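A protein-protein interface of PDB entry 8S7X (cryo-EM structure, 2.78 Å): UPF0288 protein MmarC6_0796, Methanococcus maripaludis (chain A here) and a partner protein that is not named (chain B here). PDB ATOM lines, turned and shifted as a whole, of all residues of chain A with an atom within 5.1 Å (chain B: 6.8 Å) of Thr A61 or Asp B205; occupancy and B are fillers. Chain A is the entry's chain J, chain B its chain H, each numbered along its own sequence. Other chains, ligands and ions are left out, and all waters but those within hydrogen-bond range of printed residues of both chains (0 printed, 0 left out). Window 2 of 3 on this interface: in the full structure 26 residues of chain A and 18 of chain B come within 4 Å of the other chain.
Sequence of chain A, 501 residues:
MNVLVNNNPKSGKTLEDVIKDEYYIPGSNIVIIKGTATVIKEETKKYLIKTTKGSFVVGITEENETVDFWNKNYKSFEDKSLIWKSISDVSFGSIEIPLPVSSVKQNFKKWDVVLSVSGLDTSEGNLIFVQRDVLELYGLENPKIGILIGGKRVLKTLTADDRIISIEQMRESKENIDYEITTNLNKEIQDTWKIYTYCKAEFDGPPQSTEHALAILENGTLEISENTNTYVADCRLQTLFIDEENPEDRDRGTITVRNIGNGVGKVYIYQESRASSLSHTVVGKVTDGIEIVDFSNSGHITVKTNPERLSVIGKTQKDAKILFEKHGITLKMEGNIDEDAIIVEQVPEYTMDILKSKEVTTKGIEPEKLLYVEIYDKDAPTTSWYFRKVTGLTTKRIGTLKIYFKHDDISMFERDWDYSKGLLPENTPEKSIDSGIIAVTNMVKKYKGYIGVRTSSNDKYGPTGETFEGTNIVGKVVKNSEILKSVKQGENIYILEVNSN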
ATOM      1  N   LYS A  45       2.618 -12.174 -14.546  1.00  0.00           N
ATOM      2  CA  LYS A  45       3.387 -13.403 -14.403  1.00  0.00           C
ATOM      3  C   LYS A  45       4.110 -13.718 -15.704  1.00  0.00           C
ATOM      4  O   LYS A  45       5.214 -14.273 -15.696  1.00  0.00           O
ATOM      5  CB  LYS A  45       2.472 -14.558 -13.996  1.00  0.00           C
ATOM      6  CG  LYS A  45       2.296 -14.724 -12.497  1.00  0.00           C
ATOM      7  CD  LYS A  45       3.252 -15.759 -11.938  1.00  0.00           C
ATOM      8  CE  LYS A  45       2.611 -17.138 -11.915  1.00  0.00           C
ATOM      9  NZ  LYS A  45       3.573 -18.193 -11.494  1.00  0.00           N
ATOM     10  N   GLY A  59       7.937 -15.604 -18.887  1.00  0.00           N
ATOM     11  CA  GLY A  59       6.997 -15.835 -17.805  1.00  0.00           C
ATOM     12  C   GLY A  59       7.661 -16.285 -16.521  1.00  0.00           C
ATOM     13  O   GLY A  59       8.344 -17.313 -16.502  1.00  0.00           O
ATOM     14  N   ILE A  60       7.453 -15.537 -15.436  1.00  0.00           N
ATOM     15  CA  ILE A  60       8.150 -15.834 -14.195  1.00  0.00           C
ATOM     16  C   ILE A  60       7.473 -17.007 -13.498  1.00  0.00           C
ATOM     17  O   ILE A  60       6.246 -17.044 -13.336  1.00  0.00           O
ATOM     18  CB  ILE A  60       8.228 -14.578 -13.306  1.00  0.00           C
ATOM     19  CG1 ILE A  60       6.851 -14.132 -12.808  1.00  0.00           C
ATOM     20  CG2 ILE A  60       8.890 -13.442 -14.063  1.00  0.00           C
ATOM     21  CD1 ILE A  60       6.568 -14.520 -11.370  1.00  0.00           C
ATOM     22  N   THR A  61       8.278 -18.006 -13.127  1.00  0.00           N
ATOM     23  CA  THR A  61       7.758 -19.206 -12.487  1.00  0.00           C
ATOM     24  C   THR A  61       8.293 -19.361 -11.068  1.00  0.00           C
ATOM     25  O   THR A  61       7.516 -19.430 -10.109  1.00  0.00           O
ATOM     26  CB  THR A  61       8.107 -20.443 -13.316  1.00  0.00           C
ATOM     27  OG1 THR A  61       9.524 -20.500 -13.520  1.00  0.00           O
ATOM     28  CG2 THR A  61       7.410 -20.393 -14.666  1.00  0.00           C
ATOM     29  N   GLU A  62       9.615 -19.394 -10.923  1.00  0.00           N
ATOM     30  CA  GLU A  62      10.243 -19.621  -9.624  1.00  0.00           C
ATOM     31  C   GLU A  62      10.333 -18.296  -8.881  1.00  0.00           C
ATOM     32  O   GLU A  62      10.952 -17.345  -9.369  1.00  0.00           O
ATOM     33  CB  GLU A  62      11.624 -20.245  -9.800  1.00  0.00           C
ATOM     34  CG  GLU A  62      12.428 -20.366  -8.514  1.00  0.00           C
ATOM     35  CD  GLU A  62      11.604 -20.886  -7.352  1.00  0.00           C
ATOM     36  OE1 GLU A  62      11.247 -22.083  -7.360  1.00  0.00           O
ATOM     37  OE2 GLU A  62      11.312 -20.097  -6.428  1.00  0.00           O
ATOM     38  N   GLU A  63       9.723 -18.234  -7.696  1.00  0.00           N
ATOM     39  CA  GLU A  63       9.716 -16.996  -6.923  1.00  0.00           C
ATOM     40  C   GLU A  63      11.133 -16.609  -6.504  1.00  0.00           C
ATOM     41  O   GLU A  63      11.660 -15.579  -6.936  1.00  0.00           O
ATOM     42  CB  GLU A  63       8.784 -17.149  -5.712  1.00  0.00           C
ATOM     43  CG  GLU A  63       9.195 -16.391  -4.452  1.00  0.00           C
ATOM     44  CD  GLU A  63       8.810 -14.926  -4.494  1.00  0.00           C
ATOM     45  OE1 GLU A  63       8.094 -14.521  -5.432  1.00  0.00           O
ATOM     46  OE2 GLU A  63       9.222 -14.177  -3.582  1.00  0.00           O
ATOM     47  N   LYS A 144      17.483 -18.178 -11.316  1.00  0.00           N
ATOM     48  CA  LYS A 144      16.217 -18.584 -11.913  1.00  0.00           C
ATOM     49  C   LYS A 144      15.080 -17.630 -11.562  1.00  0.00           C
ATOM     50  O   LYS A 144      14.725 -17.492 -10.387  1.00  0.00           O
ATOM     51  CB  LYS A 144      15.869 -20.000 -11.453  1.00  0.00           C
ATOM     52  CG  LYS A 144      14.529 -20.520 -11.930  1.00  0.00           C
ATOM     53  CD  LYS A 144      14.693 -21.487 -13.082  1.00  0.00           C
ATOM     54  CE  LYS A 144      13.526 -22.462 -13.150  1.00  0.00           C
ATOM     55  NZ  LYS A 144      12.307 -21.932 -12.482  1.00  0.00           N
ATOM     56  N   ILE A 145      14.504 -16.969 -12.562  1.00  0.00           N
ATOM     57  CA  ILE A 145      13.383 -16.061 -12.360  1.00  0.00           C
ATOM     58  C   ILE A 145      12.152 -16.501 -13.143  1.00  0.00           C
ATOM     59  O   ILE A 145      11.043 -16.516 -12.601  1.00  0.00           O
ATOM     60  CB  ILE A 145      13.773 -14.607 -12.713  1.00  0.00           C
ATOM     61  CG1 ILE A 145      12.537 -13.794 -13.112  1.00  0.00           C
ATOM     62  CG2 ILE A 145      14.857 -14.577 -13.778  1.00  0.00           C
ATOM     63  CD1 ILE A 145      12.582 -13.212 -14.504  1.00  0.00           C
ATOM     64  N   GLY A 146      12.321 -16.870 -14.411  1.00  0.00           N
ATOM     65  CA  GLY A 146      11.195 -17.247 -15.243  1.00  0.00           C
ATOM     66  C   GLY A 146      11.558 -18.158 -16.396  1.00  0.00           C
ATOM     67  O   GLY A 146      12.690 -18.634 -16.479  1.00  0.00           O
ATOM     68  N   ILE A 147      10.607 -18.420 -17.292  1.00  0.00           N
ATOM     69  CA  ILE A 147      10.824 -19.300 -18.434  1.00  0.00           C
ATOM     70  C   ILE A 147      10.405 -18.575 -19.708  1.00  0.00           C
ATOM     71  O   ILE A 147       9.312 -18.000 -19.771  1.00  0.00           O
ATOM     72  CB  ILE A 147      10.057 -20.629 -18.286  1.00  0.00           C
ATOM     73  CG1 ILE A 147      10.380 -21.289 -16.941  1.00  0.00           C
ATOM     74  CG2 ILE A 147      10.397 -21.572 -19.427  1.00  0.00           C
ATOM     75  CD1 ILE A 147      10.011 -22.762 -16.860  1.00  0.00           C
ATOM     76  N   THR B 200       3.621 -30.123  -8.088  1.00  0.00           N
ATOM     77  CA  THR B 200       2.653 -29.047  -8.267  1.00  0.00           C
ATOM     78  C   THR B 200       3.303 -27.817  -8.885  1.00  0.00           C
ATOM     79  O   THR B 200       2.729 -27.180  -9.773  1.00  0.00           O
ATOM     80  CB  THR B 200       2.016 -28.692  -6.925  1.00  0.00           C
ATOM     81  OG1 THR B 200       1.190 -29.773  -6.486  1.00  0.00           O
ATOM     82  CG2 THR B 200       1.168 -27.441  -7.049  1.00  0.00           C
ATOM     83  N   LYS B 201       4.504 -27.462  -8.421  1.00  0.00           N
ATOM     84  CA  LYS B 201       5.203 -26.317  -8.994  1.00  0.00           C
ATOM     85  C   LYS B 201       5.516 -26.547 -10.466  1.00  0.00           C
ATOM     86  O   LYS B 201       5.306 -25.657 -11.301  1.00  0.00           O
ATOM     87  CB  LYS B 201       6.481 -26.042  -8.209  1.00  0.00           C
ATOM     88  CG  LYS B 201       7.429 -25.067  -8.879  1.00  0.00           C
ATOM     89  CD  LYS B 201       8.709 -24.921  -8.077  1.00  0.00           C
ATOM     90  CE  LYS B 201       8.454 -24.212  -6.757  1.00  0.00           C
ATOM     91  NZ  LYS B 201       8.454 -25.157  -5.607  1.00  0.00           N
ATOM     92  N   LYS B 202       6.012 -27.739 -10.806  1.00  0.00           N
ATOM     93  CA  LYS B 202       6.318 -28.022 -12.206  1.00  0.00           C
ATOM     94  C   LYS B 202       5.058 -27.977 -13.065  1.00  0.00           C
ATOM     95  O   LYS B 202       5.074 -27.448 -14.183  1.00  0.00           O
ATOM     96  CB  LYS B 202       7.010 -29.378 -12.328  1.00  0.00           C
ATOM     97  CG  LYS B 202       8.296 -29.477 -11.531  1.00  0.00           C
ATOM     98  CD  LYS B 202       9.276 -30.444 -12.169  1.00  0.00           C
ATOM     99  CE  LYS B 202      10.704 -30.068 -11.832  1.00  0.00           C
ATOM    100  NZ  LYS B 202      11.659 -30.551 -12.863  1.00  0.00           N
ATOM    101  N   ILE B 203       3.949 -28.516 -12.550  1.00  0.00           N
ATOM    102  CA  ILE B 203       2.700 -28.529 -13.302  1.00  0.00           C
ATOM    103  C   ILE B 203       2.159 -27.117 -13.489  1.00  0.00           C
ATOM    104  O   ILE B 203       1.642 -26.783 -14.558  1.00  0.00           O
ATOM    105  CB  ILE B 203       1.679 -29.457 -12.620  1.00  0.00           C
ATOM    106  CG1 ILE B 203       1.663 -30.822 -13.310  1.00  0.00           C
ATOM    107  CG2 ILE B 203       0.287 -28.843 -12.602  1.00  0.00           C
ATOM    108  CD1 ILE B 203       3.010 -31.474 -13.431  1.00  0.00           C
ATOM    109  N   ASN B 204       2.267 -26.265 -12.468  1.00  0.00           N
ATOM    110  CA  ASN B 204       1.813 -24.887 -12.621  1.00  0.00           C
ATOM    111  C   ASN B 204       2.671 -24.127 -13.627  1.00  0.00           C
ATOM    112  O   ASN B 204       2.155 -23.324 -14.417  1.00  0.00           O
ATOM    113  CB  ASN B 204       1.805 -24.184 -11.267  1.00  0.00           C
ATOM    114  CG  ASN B 204       0.563 -24.490 -10.468  1.00  0.00           C
ATOM    115  OD1 ASN B 204      -0.166 -25.427 -10.781  1.00  0.00           O
ATOM    116  ND2 ASN B 204       0.314 -23.705  -9.429  1.00  0.00           N
ATOM    117  N   ASP B 205       3.983 -24.369 -13.619  1.00  0.00           N
ATOM    118  CA  ASP B 205       4.833 -23.777 -14.646  1.00  0.00           C
ATOM    119  C   ASP B 205       4.387 -24.210 -16.037  1.00  0.00           C
ATOM    120  O   ASP B 205       4.201 -23.373 -16.930  1.00  0.00           O
ATOM    121  CB  ASP B 205       6.295 -24.155 -14.403  1.00  0.00           C
ATOM    122  CG  ASP B 205       6.804 -23.689 -13.054  1.00  0.00           C
ATOM    123  OD1 ASP B 205       6.060 -22.971 -12.355  1.00  0.00           O
ATOM    124  OD2 ASP B 205       7.946 -24.039 -12.693  1.00  0.00           O
ATOM    125  N   LYS B 206       4.185 -25.516 -16.230  1.00  0.00           N
ATOM    126  CA  LYS B 206       3.747 -26.013 -17.533  1.00  0.00           C
ATOM    127  C   LYS B 206       2.380 -25.455 -17.905  1.00  0.00           C
ATOM    128  O   LYS B 206       2.089 -25.230 -19.086  1.00  0.00           O
ATOM    129  CB  LYS B 206       3.722 -27.540 -17.532  1.00  0.00           C
ATOM    130  CG  LYS B 206       3.560 -28.161 -18.910  1.00  0.00           C
ATOM    131  CD  LYS B 206       4.863 -28.161 -19.686  1.00  0.00           C
ATOM    132  CE  LYS B 206       6.012 -28.686 -18.846  1.00  0.00           C
ATOM    133  NZ  LYS B 206       7.312 -28.068 -19.224  1.00  0.00           N
ATOM    134  N   ARG B 207       1.531 -25.222 -16.907  1.00  0.00           N
ATOM    135  CA  ARG B 207       0.235 -24.610 -17.165  1.00  0.00           C
ATOM    136  C   ARG B 207       0.402 -23.195 -17.697  1.00  0.00           C
ATOM    137  O   ARG B 207      -0.329 -22.773 -18.595  1.00  0.00           O
ATOM    138  CB  ARG B 207      -0.611 -24.616 -15.892  1.00  0.00           C
ATOM    139  CG  ARG B 207      -1.858 -25.468 -16.002  1.00  0.00           C
ATOM    140  CD  ARG B 207      -2.879 -25.121 -14.931  1.00  0.00           C
ATOM    141  NE  ARG B 207      -2.739 -25.954 -13.743  1.00  0.00           N
ATOM    142  CZ  ARG B 207      -3.056 -27.241 -13.684  1.00  0.00           C
ATOM    143  NH1 ARG B 207      -3.523 -27.889 -14.739  1.00  0.00           N
ATOM    144  NH2 ARG B 207      -2.901 -27.895 -12.536  1.00  0.00           N
ATOM    145  N   MET B 208       1.361 -22.447 -17.151  1.00  0.00           N
ATOM    146  CA  MET B 208       1.640 -21.118 -17.694  1.00  0.00           C
ATOM    147  C   MET B 208       2.177 -21.202 -19.120  1.00  0.00           C
ATOM    148  O   MET B 208       1.766 -20.423 -19.994  1.00  0.00           O
ATOM    149  CB  MET B 208       2.612 -20.367 -16.788  1.00  0.00           C
ATOM    150  CG  MET B 208       2.028 -19.727 -15.505  1.00  0.00           C
ATOM    151  SD  MET B 208       0.394 -18.925 -15.489  1.00  0.00           S
ATOM    152  CE  MET B 208      -0.782 -20.278 -15.597  1.00  0.00           C
ATOM    153  N   GLU B 209       3.098 -22.141 -19.377  1.00  0.00           N
ATOM    154  CA  GLU B 209       3.546 -22.363 -20.754  1.00  0.00           C
ATOM    155  C   GLU B 209       2.369 -22.583 -21.692  1.00  0.00           C
ATOM    156  O   GLU B 209       2.306 -21.986 -22.773  1.00  0.00           O
ATOM    157  CB  GLU B 209       4.515 -23.547 -20.864  1.00  0.00           C
ATOM    158  CG  GLU B 209       5.995 -23.201 -20.767  1.00  0.00           C
ATOM    159  CD  GLU B 209       6.680 -23.600 -19.478  1.00  0.00           C
ATOM    160  OE1 GLU B 209       6.008 -24.085 -18.557  1.00  0.00           O
ATOM    161  OE2 GLU B 209       7.911 -23.412 -19.387  1.00  0.00           O
ATOM    162  N   LEU B 210       1.427 -23.439 -21.299  1.00  0.00           N
ATOM    163  CA  LEU B 210       0.271 -23.701 -22.152  1.00  0.00           C
ATOM    164  C   LEU B 210      -0.613 -22.466 -22.280  1.00  0.00           C
ATOM    165  O   LEU B 210      -1.177 -22.205 -23.349  1.00  0.00           O
ATOM    166  CB  LEU B 210      -0.525 -24.884 -21.607  1.00  0.00           C
ATOM    167  CG  LEU B 210      -0.259 -26.203 -22.330  1.00  0.00           C
ATOM    168  CD1 LEU B 210      -0.513 -26.047 -23.817  1.00  0.00           C
ATOM    169  CD2 LEU B 210       1.159 -26.685 -22.076  1.00  0.00           C
ATOM    170  N   SER B 211      -0.747 -21.693 -21.201  1.00  0.00           N
ATOM    171  CA  SER B 211      -1.592 -20.508 -21.223  1.00  0.00           C
ATOM    172  C   SER B 211      -1.023 -19.400 -22.094  1.00  0.00           C
ATOM    173  O   SER B 211      -1.769 -18.496 -22.486  1.00  0.00           O
ATOM    174  CB  SER B 211      -1.809 -19.985 -19.805  1.00  0.00           C
ATOM    175  OG  SER B 211      -2.420 -18.707 -19.825  1.00  0.00           O
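NZ of Lys A144 sits at hydrogen-bond distance from OG1 of Thr A61, 3.3 Å away.
N of Lys B206 sits close to OE1 of Glu B209, 3.3 Å away.
The backbone carbonyl oxygen (O) of Gly A59 lies within hydrogen-bond range of the backbone NH (N) of Ile A147, at 2.6 Å.
The backbone NH (N) of Thr A61 sits at hydrogen-bond distance from the backbone carbonyl oxygen (O) of Ile A145 (3.2 Å).
The side-chain carboxylate (OE1) of Glu B209 sits close to the backbone carbonyl oxygen (O) of Asp B205.
Among the printed residues, merely in contact across the chains: Ile A147 with Glu B209 (3.1 Å), Thr A61 with Asp B205 (3.4 Å) and Glu A62 with Lys B201 (3.6 Å).
Of chain B, only Asp B205 (3.4 Å) comes within 4 Å of Thr A61.
Printed residues of chain B within 4 Å of Glu A62: Lys B201.
Printed residues of chain A within 4 Å of Lys B201: Glu A62.
Of the printed residues of chain A, Glu B209 touches Ile A147.
The nearest residue of chain B that does not touch Thr A61 is Met B208 (5.2 Å).
Of the 10 printed residues of chain A, 3 touch a printed residue of chain B.
Among the printed residues, no Asp or Glu carboxylate lies within 4 Å of a Lys or Arg side-chain nitrogen of the other chain.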
